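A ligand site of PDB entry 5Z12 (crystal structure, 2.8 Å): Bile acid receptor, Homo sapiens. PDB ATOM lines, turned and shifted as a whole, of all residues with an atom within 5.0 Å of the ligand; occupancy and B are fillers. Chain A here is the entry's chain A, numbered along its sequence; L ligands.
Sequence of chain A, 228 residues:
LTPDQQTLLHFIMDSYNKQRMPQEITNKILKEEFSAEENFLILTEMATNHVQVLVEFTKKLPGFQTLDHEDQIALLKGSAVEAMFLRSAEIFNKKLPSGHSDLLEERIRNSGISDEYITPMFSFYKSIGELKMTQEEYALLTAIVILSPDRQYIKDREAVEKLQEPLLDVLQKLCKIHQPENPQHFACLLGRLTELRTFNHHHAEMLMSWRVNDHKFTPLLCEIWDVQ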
ATOM      1  N   ILE A  25      28.938  16.572  -5.157  1.00  0.00           N
ATOM      2  CA  ILE A  25      28.015  16.248  -6.244  1.00  0.00           C
ATOM      3  C   ILE A  25      28.592  16.767  -7.567  1.00  0.00           C
ATOM      4  O   ILE A  25      28.826  15.992  -8.503  1.00  0.00           O
ATOM      5  CB  ILE A  25      26.613  16.862  -5.959  1.00  0.00           C
ATOM      6  CG1 ILE A  25      25.973  16.270  -4.683  1.00  0.00           C
ATOM      7  CG2 ILE A  25      25.674  16.736  -7.152  1.00  0.00           C
ATOM      8  CD1 ILE A  25      25.653  14.793  -4.741  1.00  0.00           C
ATOM      9  N   THR A  26      28.819  18.077  -7.624  1.00  0.00           N
ATOM     10  CA  THR A  26      29.455  18.733  -8.762  1.00  0.00           C
ATOM     11  C   THR A  26      30.598  17.861  -9.278  1.00  0.00           C
ATOM     12  O   THR A  26      30.609  17.475 -10.442  1.00  0.00           O
ATOM     13  CB  THR A  26      29.933  20.140  -8.340  1.00  0.00           C
ATOM     14  OG1 THR A  26      28.850  21.065  -8.514  1.00  0.00           O
ATOM     15  CG2 THR A  26      31.155  20.656  -9.156  1.00  0.00           C
ATOM     16  N   ILE A  29      30.157  14.398 -11.377  1.00  0.00           N
ATOM     17  CA  ILE A  29      29.744  14.495 -12.787  1.00  0.00           C
ATOM     18  C   ILE A  29      30.759  15.152 -13.716  1.00  0.00           C
ATOM     19  O   ILE A  29      30.989  14.639 -14.822  1.00  0.00           O
ATOM     20  CB  ILE A  29      28.388  15.185 -12.947  1.00  0.00           C
ATOM     21  CG1 ILE A  29      27.299  14.218 -12.484  1.00  0.00           C
ATOM     22  CG2 ILE A  29      28.113  15.560 -14.411  1.00  0.00           C
ATOM     23  CD1 ILE A  29      25.930  14.817 -12.294  1.00  0.00           C
ATOM     24  N   PHE A  40      24.121   7.683 -16.349  1.00  0.00           N
ATOM     25  CA  PHE A  40      22.939   7.123 -15.724  1.00  0.00           C
ATOM     26  C   PHE A  40      23.272   6.484 -14.375  1.00  0.00           C
ATOM     27  O   PHE A  40      22.639   6.775 -13.369  1.00  0.00           O
ATOM     28  CB  PHE A  40      22.243   6.121 -16.632  1.00  0.00           C
ATOM     29  CG  PHE A  40      20.806   5.880 -16.276  1.00  0.00           C
ATOM     30  CD1 PHE A  40      19.817   6.827 -16.598  1.00  0.00           C
ATOM     31  CD2 PHE A  40      20.420   4.712 -15.598  1.00  0.00           C
ATOM     32  CE1 PHE A  40      18.485   6.607 -16.255  1.00  0.00           C
ATOM     33  CE2 PHE A  40      19.091   4.481 -15.263  1.00  0.00           C
ATOM     34  CZ  PHE A  40      18.116   5.424 -15.589  1.00  0.00           C
ATOM     35  N   LEU A  43      24.091   9.396 -11.833  1.00  0.00           N
ATOM     36  CA  LEU A  43      22.853  10.099 -11.469  1.00  0.00           C
ATOM     37  C   LEU A  43      21.940   9.236 -10.595  1.00  0.00           C
ATOM     38  O   LEU A  43      21.353   9.730  -9.623  1.00  0.00           O
ATOM     39  CB  LEU A  43      22.105  10.546 -12.719  1.00  0.00           C
ATOM     40  CG  LEU A  43      22.751  11.644 -13.548  1.00  0.00           C
ATOM     41  CD1 LEU A  43      21.931  11.859 -14.807  1.00  0.00           C
ATOM     42  CD2 LEU A  43      22.869  12.951 -12.788  1.00  0.00           C
ATOM     43  N   THR A  44      21.847   7.959 -10.946  1.00  0.00           N
ATOM     44  CA  THR A  44      21.123   6.982 -10.175  1.00  0.00           C
ATOM     45  C   THR A  44      21.607   6.998  -8.722  1.00  0.00           C
ATOM     46  O   THR A  44      20.811   7.178  -7.801  1.00  0.00           O
ATOM     47  CB  THR A  44      21.222   5.601 -10.863  1.00  0.00           C
ATOM     48  OG1 THR A  44      20.450   5.618 -12.068  1.00  0.00           O
ATOM     49  CG2 THR A  44      20.692   4.475  -9.997  1.00  0.00           C
ATOM     50  N   MET A  46      23.426   9.279  -7.048  1.00  0.00           N
ATOM     51  CA  MET A  46      23.214  10.557  -6.371  1.00  0.00           C
ATOM     52  C   MET A  46      21.805  10.628  -5.763  1.00  0.00           C
ATOM     53  O   MET A  46      21.620  10.947  -4.559  1.00  0.00           O
ATOM     54  CB  MET A  46      23.366  11.688  -7.388  1.00  0.00           C
ATOM     55  CG  MET A  46      24.771  11.988  -7.834  1.00  0.00           C
ATOM     56  SD  MET A  46      24.707  13.348  -9.009  1.00  0.00           S
ATOM     57  CE  MET A  46      26.466  13.745  -9.008  1.00  0.00           C
ATOM     58  N   ALA A  47      20.817  10.326  -6.623  1.00  0.00           N
ATOM     59  CA  ALA A  47      19.386  10.329  -6.262  1.00  0.00           C
ATOM     60  C   ALA A  47      19.094   9.354  -5.156  1.00  0.00           C
ATOM     61  O   ALA A  47      18.307   9.641  -4.286  1.00  0.00           O
ATOM     62  CB  ALA A  47      18.541   9.982  -7.464  1.00  0.00           C
ATOM     63  N   HIS A  50      20.543  11.010  -2.137  1.00  0.00           N
ATOM     64  CA  HIS A  50      19.616  12.084  -1.779  1.00  0.00           C
ATOM     65  C   HIS A  50      18.400  11.552  -1.015  1.00  0.00           C
ATOM     66  O   HIS A  50      18.016  12.137   0.011  1.00  0.00           O
ATOM     67  CB  HIS A  50      19.159  12.878  -3.007  1.00  0.00           C
ATOM     68  CG  HIS A  50      18.143  13.925  -2.684  1.00  0.00           C
ATOM     69  ND1 HIS A  50      18.444  15.046  -1.935  1.00  0.00           N
ATOM     70  CD2 HIS A  50      16.821  13.998  -2.953  1.00  0.00           C
ATOM     71  CE1 HIS A  50      17.348  15.768  -1.761  1.00  0.00           C
ATOM     72  NE2 HIS A  50      16.345  15.153  -2.371  1.00  0.00           N
ATOM     73  N   MET A  84      14.144  16.650  -4.785  1.00  0.00           N
ATOM     74  CA  MET A  84      15.389  16.445  -5.521  1.00  0.00           C
ATOM     75  C   MET A  84      15.673  17.633  -6.414  1.00  0.00           C
ATOM     76  O   MET A  84      16.824  18.119  -6.421  1.00  0.00           O
ATOM     77  CB  MET A  84      15.340  15.179  -6.366  1.00  0.00           C
ATOM     78  CG  MET A  84      16.521  15.060  -7.308  1.00  0.00           C
ATOM     79  SD  MET A  84      16.580  13.505  -8.198  1.00  0.00           S
ATOM     80  CE  MET A  84      15.308  13.722  -9.429  1.00  0.00           C
ATOM     81  N   PHE A  85      14.666  18.077  -7.181  1.00  0.00           N
ATOM     82  CA  PHE A  85      14.872  19.139  -8.166  1.00  0.00           C
ATOM     83  C   PHE A  85      15.219  20.438  -7.494  1.00  0.00           C
ATOM     84  O   PHE A  85      16.048  21.175  -7.983  1.00  0.00           O
ATOM     85  CB  PHE A  85      13.670  19.309  -9.076  1.00  0.00           C
ATOM     86  CG  PHE A  85      13.649  18.322 -10.180  1.00  0.00           C
ATOM     87  CD1 PHE A  85      14.517  18.462 -11.248  1.00  0.00           C
ATOM     88  CD2 PHE A  85      12.804  17.223 -10.147  1.00  0.00           C
ATOM     89  CE1 PHE A  85      14.541  17.535 -12.278  1.00  0.00           C
ATOM     90  CE2 PHE A  85      12.822  16.287 -11.168  1.00  0.00           C
ATOM     91  CZ  PHE A  85      13.685  16.448 -12.243  1.00  0.00           C
ATOM     92  N   ARG A  87      16.868  20.675  -4.675  1.00  0.00           N
ATOM     93  CA  ARG A  87      18.260  20.489  -4.273  1.00  0.00           C
ATOM     94  C   ARG A  87      19.252  20.570  -5.422  1.00  0.00           C
ATOM     95  O   ARG A  87      20.365  21.006  -5.243  1.00  0.00           O
ATOM     96  CB  ARG A  87      18.444  19.148  -3.582  1.00  0.00           C
ATOM     97  CG  ARG A  87      19.847  18.811  -3.133  1.00  0.00           C
ATOM     98  CD  ARG A  87      20.392  19.844  -2.166  1.00  0.00           C
ATOM     99  NE  ARG A  87      21.744  19.494  -1.733  1.00  0.00           N
ATOM    100  CZ  ARG A  87      22.609  20.308  -1.124  1.00  0.00           C
ATOM    101  NH1 ARG A  87      22.288  21.563  -0.834  1.00  0.00           N
ATOM    102  NH2 ARG A  87      23.824  19.851  -0.798  1.00  0.00           N
ATOM    103  N   SER A  88      18.849  20.085  -6.586  1.00  0.00           N
ATOM    104  CA  SER A  88      19.644  20.245  -7.819  1.00  0.00           C
ATOM    105  C   SER A  88      19.778  21.720  -8.173  1.00  0.00           C
ATOM    106  O   SER A  88      20.858  22.209  -8.528  1.00  0.00           O
ATOM    107  CB  SER A  88      18.957  19.517  -8.974  1.00  0.00           C
ATOM    108  OG  SER A  88      18.552  18.236  -8.580  1.00  0.00           O
ATOM    109  N   ILE A  91      22.199  23.268  -6.057  1.00  0.00           N
ATOM    110  CA  ILE A  91      23.563  22.868  -6.428  1.00  0.00           C
ATOM    111  C   ILE A  91      24.003  23.556  -7.722  1.00  0.00           C
ATOM    112  O   ILE A  91      25.046  24.201  -7.752  1.00  0.00           O
ATOM    113  CB  ILE A  91      23.663  21.322  -6.533  1.00  0.00           C
ATOM    114  CG1 ILE A  91      23.458  20.691  -5.149  1.00  0.00           C
ATOM    115  CG2 ILE A  91      25.034  20.868  -7.043  1.00  0.00           C
ATOM    116  CD1 ILE A  91      22.973  19.253  -5.217  1.00  0.00           C
ATOM    117  N   PHE A  92      23.206  23.428  -8.761  1.00  0.00           N
ATOM    118  CA  PHE A  92      23.491  24.062 -10.064  1.00  0.00           C
ATOM    119  C   PHE A  92      23.829  25.565 -10.012  1.00  0.00           C
ATOM    120  O   PHE A  92      24.676  26.041 -10.781  1.00  0.00           O
ATOM    121  CB  PHE A  92      22.299  23.881 -11.008  1.00  0.00           C
ATOM    122  CG  PHE A  92      22.569  24.262 -12.436  1.00  0.00           C
ATOM    123  CD1 PHE A  92      23.429  23.490 -13.219  1.00  0.00           C
ATOM    124  CD2 PHE A  92      21.941  25.356 -13.011  1.00  0.00           C
ATOM    125  CE1 PHE A  92      23.671  23.833 -14.551  1.00  0.00           C
ATOM    126  CE2 PHE A  92      22.161  25.703 -14.345  1.00  0.00           C
ATOM    127  CZ  PHE A  92      23.040  24.939 -15.118  1.00  0.00           C
ATOM    128  N   LEU A 104      28.872  21.438 -16.833  1.00  0.00           N
ATOM    129  CA  LEU A 104      27.956  20.618 -16.062  1.00  0.00           C
ATOM    130  C   LEU A 104      26.646  20.493 -16.838  1.00  0.00           C
ATOM    131  O   LEU A 104      26.167  19.387 -17.060  1.00  0.00           O
ATOM    132  CB  LEU A 104      27.716  21.276 -14.696  1.00  0.00           C
ATOM    133  CG  LEU A 104      26.806  20.610 -13.669  1.00  0.00           C
ATOM    134  CD1 LEU A 104      27.373  19.268 -13.259  1.00  0.00           C
ATOM    135  CD2 LEU A 104      26.621  21.529 -12.474  1.00  0.00           C
ATOM    136  N   ILE A 108      24.869  16.964 -18.343  1.00  0.00           N
ATOM    137  CA  ILE A 108      23.538  16.482 -17.961  1.00  0.00           C
ATOM    138  C   ILE A 108      22.691  16.303 -19.220  1.00  0.00           C
ATOM    139  O   ILE A 108      21.959  15.317 -19.308  1.00  0.00           O
ATOM    140  CB  ILE A 108      22.843  17.443 -17.001  1.00  0.00           C
ATOM    141  CG1 ILE A 108      23.600  17.500 -15.678  1.00  0.00           C
ATOM    142  CG2 ILE A 108      21.403  17.023 -16.717  1.00  0.00           C
ATOM    143  CD1 ILE A 108      23.321  18.778 -14.910  1.00  0.00           C
ATOM    144  N   ILE A 113      18.485  11.425 -21.371  1.00  0.00           N
ATOM    145  CA  ILE A 113      17.210  12.067 -21.076  1.00  0.00           C
ATOM    146  C   ILE A 113      16.924  13.052 -22.216  1.00  0.00           C
ATOM    147  O   ILE A 113      17.839  13.657 -22.759  1.00  0.00           O
ATOM    148  CB  ILE A 113      17.214  12.724 -19.684  1.00  0.00           C
ATOM    149  CG1 ILE A 113      17.242  11.650 -18.584  1.00  0.00           C
ATOM    150  CG2 ILE A 113      15.976  13.549 -19.449  1.00  0.00           C
ATOM    151  CD1 ILE A 113      18.537  11.554 -17.810  1.00  0.00           C
ATOM    152  N   MET A 121      14.027  21.831 -16.950  1.00  0.00           N
ATOM    153  CA  MET A 121      14.838  21.839 -15.727  1.00  0.00           C
ATOM    154  C   MET A 121      15.714  23.057 -15.611  1.00  0.00           C
ATOM    155  O   MET A 121      15.684  23.760 -14.601  1.00  0.00           O
ATOM    156  CB  MET A 121      15.762  20.666 -15.693  1.00  0.00           C
ATOM    157  CG  MET A 121      15.104  19.359 -15.430  1.00  0.00           C
ATOM    158  SD  MET A 121      16.432  18.164 -15.272  1.00  0.00           S
ATOM    159  CE  MET A 121      15.482  16.787 -15.976  1.00  0.00           C
ATOM    160  N   TYR A 125      15.932  25.849 -12.881  1.00  0.00           N
ATOM    161  CA  TYR A 125      17.191  26.152 -12.157  1.00  0.00           C
ATOM    162  C   TYR A 125      17.595  27.602 -12.360  1.00  0.00           C
ATOM    163  O   TYR A 125      17.930  28.274 -11.413  1.00  0.00           O
ATOM    164  CB  TYR A 125      18.357  25.224 -12.567  1.00  0.00           C
ATOM    165  CG  TYR A 125      18.158  23.715 -12.385  1.00  0.00           C
ATOM    166  CD1 TYR A 125      17.282  23.190 -11.424  1.00  0.00           C
ATOM    167  CD2 TYR A 125      18.893  22.815 -13.146  1.00  0.00           C
ATOM    168  CE1 TYR A 125      17.131  21.813 -11.274  1.00  0.00           C
ATOM    169  CE2 TYR A 125      18.752  21.434 -13.013  1.00  0.00           C
ATOM    170  CZ  TYR A 125      17.876  20.928 -12.067  1.00  0.00           C
ATOM    171  OH  TYR A 125      17.737  19.557 -11.935  1.00  0.00           O
ATOM    172  N   MET A 206       9.454  10.460 -17.918  1.00  0.00           N
ATOM    173  CA  MET A 206      10.807  10.874 -18.333  1.00  0.00           C
ATOM    174  C   MET A 206      11.763   9.706 -18.292  1.00  0.00           C
ATOM    175  O   MET A 206      12.521   9.479 -19.238  1.00  0.00           O
ATOM    176  CB  MET A 206      11.353  11.965 -17.412  1.00  0.00           C
ATOM    177  CG  MET A 206      12.783  12.407 -17.694  1.00  0.00           C
ATOM    178  SD  MET A 206      13.477  13.413 -16.376  1.00  0.00           S
ATOM    179  CE  MET A 206      13.962  12.127 -15.239  1.00  0.00           C
ATOM    180  N   LEU A 207      11.745   9.009 -17.173  1.00  0.00           N
ATOM    181  CA  LEU A 207      12.605   7.842 -16.954  1.00  0.00           C
ATOM    182  C   LEU A 207      12.311   6.718 -17.968  1.00  0.00           C
ATOM    183  O   LEU A 207      13.246   6.191 -18.590  1.00  0.00           O
ATOM    184  CB  LEU A 207      12.479   7.355 -15.515  1.00  0.00           C
ATOM    185  CG  LEU A 207      12.978   8.381 -14.492  1.00  0.00           C
ATOM    186  CD1 LEU A 207      12.599   7.967 -13.085  1.00  0.00           C
ATOM    187  CD2 LEU A 207      14.476   8.603 -14.586  1.00  0.00           C
ATOM    188  N   TRP A 225      10.033   6.051  -6.369  1.00  0.00           N
ATOM    189  CA  TRP A 225       9.673   6.701  -7.653  1.00  0.00           C
ATOM    190  C   TRP A 225       8.620   5.933  -8.486  1.00  0.00           C
ATOM    191  O   TRP A 225       8.137   6.476  -9.493  1.00  0.00           O
ATOM    192  CB  TRP A 225      10.922   6.921  -8.538  1.00  0.00           C
ATOM    193  CG  TRP A 225      11.916   7.983  -8.089  1.00  0.00           C
ATOM    194  CD1 TRP A 225      11.802   8.840  -7.004  1.00  0.00           C
ATOM    195  CD2 TRP A 225      13.122   8.322  -8.740  1.00  0.00           C
ATOM    196  NE1 TRP A 225      12.906   9.666  -6.939  1.00  0.00           N
ATOM    197  CE2 TRP A 225      13.725   9.367  -8.000  1.00  0.00           C
ATOM    198  CE3 TRP A 225      13.781   7.832  -9.870  1.00  0.00           C
ATOM    199  CZ2 TRP A 225      14.941   9.932  -8.371  1.00  0.00           C
ATOM    200  CZ3 TRP A 225      14.990   8.398 -10.246  1.00  0.00           C
ATOM    201  CH2 TRP A 225      15.555   9.440  -9.503  1.00  0.00           C
HETATM  202  F1  LIG L   1      24.881  16.894 -10.227  1.00  0.00           F
HETATM  203  C1  LIG L   1      23.883  17.696 -10.586  1.00  0.00           C
HETATM  204  C2  LIG L   1      24.101  19.046 -10.445  1.00  0.00           C
HETATM  205  F2  LIG L   1      25.287  19.443  -9.969  1.00  0.00           F
HETATM  206  C3  LIG L   1      23.115  19.937 -10.803  1.00  0.00           C
HETATM  207  C4  LIG L   1      21.909  19.420 -11.292  1.00  0.00           C
HETATM  208  C5  LIG L   1      22.708  17.174 -11.068  1.00  0.00           C
HETATM  209  C6  LIG L   1      21.689  18.042 -11.416  1.00  0.00           C
HETATM  210  C7  LIG L   1      20.371  17.541 -11.950  1.00  0.00           C
HETATM  211  O1  LIG L   1      19.928  18.152 -12.911  1.00  0.00           O
HETATM  212  N1  LIG L   1      19.674  16.497 -11.431  1.00  0.00           N
HETATM  213  C8  LIG L   1      18.547  15.945 -12.172  1.00  0.00           C
HETATM  214  C9  LIG L   1      18.544  14.710 -13.030  1.00  0.00           C
HETATM  215  C10 LIG L   1      19.540  14.791 -14.166  1.00  0.00           C
HETATM  216  C11 LIG L   1      17.094  14.694 -13.534  1.00  0.00           C
HETATM  217  C12 LIG L   1      18.777  13.586 -12.083  1.00  0.00           C
HETATM  218  C13 LIG L   1      18.453  12.278 -12.446  1.00  0.00           C
HETATM  219  C14 LIG L   1      17.936  11.661 -13.605  1.00  0.00           C
HETATM  220  C15 LIG L   1      17.714  10.280 -13.648  1.00  0.00           C
HETATM  221  C16 LIG L   1      19.921  16.012 -10.256  1.00  0.00           C
HETATM  222  C17 LIG L   1      19.814  14.720  -9.850  1.00  0.00           C
HETATM  223  C18 LIG L   1      20.281  14.365  -8.466  1.00  0.00           C
HETATM  224  O2  LIG L   1      21.462  14.907  -7.738  1.00  0.00           O
HETATM  225  C19 LIG L   1      21.281  15.568  -6.468  1.00  0.00           C
HETATM  226  C20 LIG L   1      20.416  16.804  -6.585  1.00  0.00           C
HETATM  227  C21 LIG L   1      20.580  14.721  -5.437  1.00  0.00           C
HETATM  228  O3  LIG L   1      19.664  13.508  -7.866  1.00  0.00           O
HETATM  229  C22 LIG L   1      19.257  13.577 -10.686  1.00  0.00           C
HETATM  230  N2  LIG L   1      19.255  12.279 -10.358  1.00  0.00           N
HETATM  231  C23 LIG L   1      18.771  11.508 -11.351  1.00  0.00           C
HETATM  232  C24 LIG L   1      18.582  10.130 -11.411  1.00  0.00           C
HETATM  233  C25 LIG L   1      18.042   9.519 -12.549  1.00  0.00           C
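The side-chain hydroxyl (OH) of Tyr 125 lies within hydrogen-bond range of an oxygen (O1) of the ligand. A nitrogen (N2) of the ligand lies within hydrogen-bond range of the side-chain sulfur of Met 84 (3.7 Å). O of Leu 43 sits close to N2 of the ligand (3.4 Å).
The side-chain hydroxyl (OG) of Ser 88 sits at hydrogen-bond distance from the backbone carbonyl oxygen (O) of Met 84, at 2.8 Å. The backbone carbonyl oxygen (O) of Phe 40 lies within hydrogen-bond range of the side-chain hydroxyl (OG1) of Thr 44 (2.8 Å).
SD of Met 46 sits close to F1 of the ligand, at 3.8 Å. Residues that only touch the ligand: Ile 25 (3.2 Å), Ile 29 (3.1 Å), Thr 44 (3.9 Å), Ala 47 (3.6 Å), His 50 (3.4 Å), Ser 88 (3.1 Å), Ile 91 (3.3 Å), Leu 104 (3.5 Å), Ile 108 (3.9 Å), Met 121 (3.6 Å), Leu 207 (3.8 Å) and Trp 225 (3.6 Å). Hydrophobic or aromatic side chains that line the ligand: Ile 25, Ile 29, Leu 43, Met 46, Ala 47, His 50, Met 84, Ile 91, Leu 104, Ile 108, Met 121, Tyr 125, Leu 207 and Trp 225. Within 4 Å of the ligand: Ile 25, Ile 29, Leu 43, Thr 44, Met 46, Ala 47, His 50, Met 84, Ser 88, Ile 91, Leu 104, Ile 108, Met 121, Tyr 125, Leu 207 and Trp 225. Along chain A the residues within 4 Å of the ligand span positions 25 to 225. The nearest printed residue that does not touch the ligand is Phe 85 (4.02 Å).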
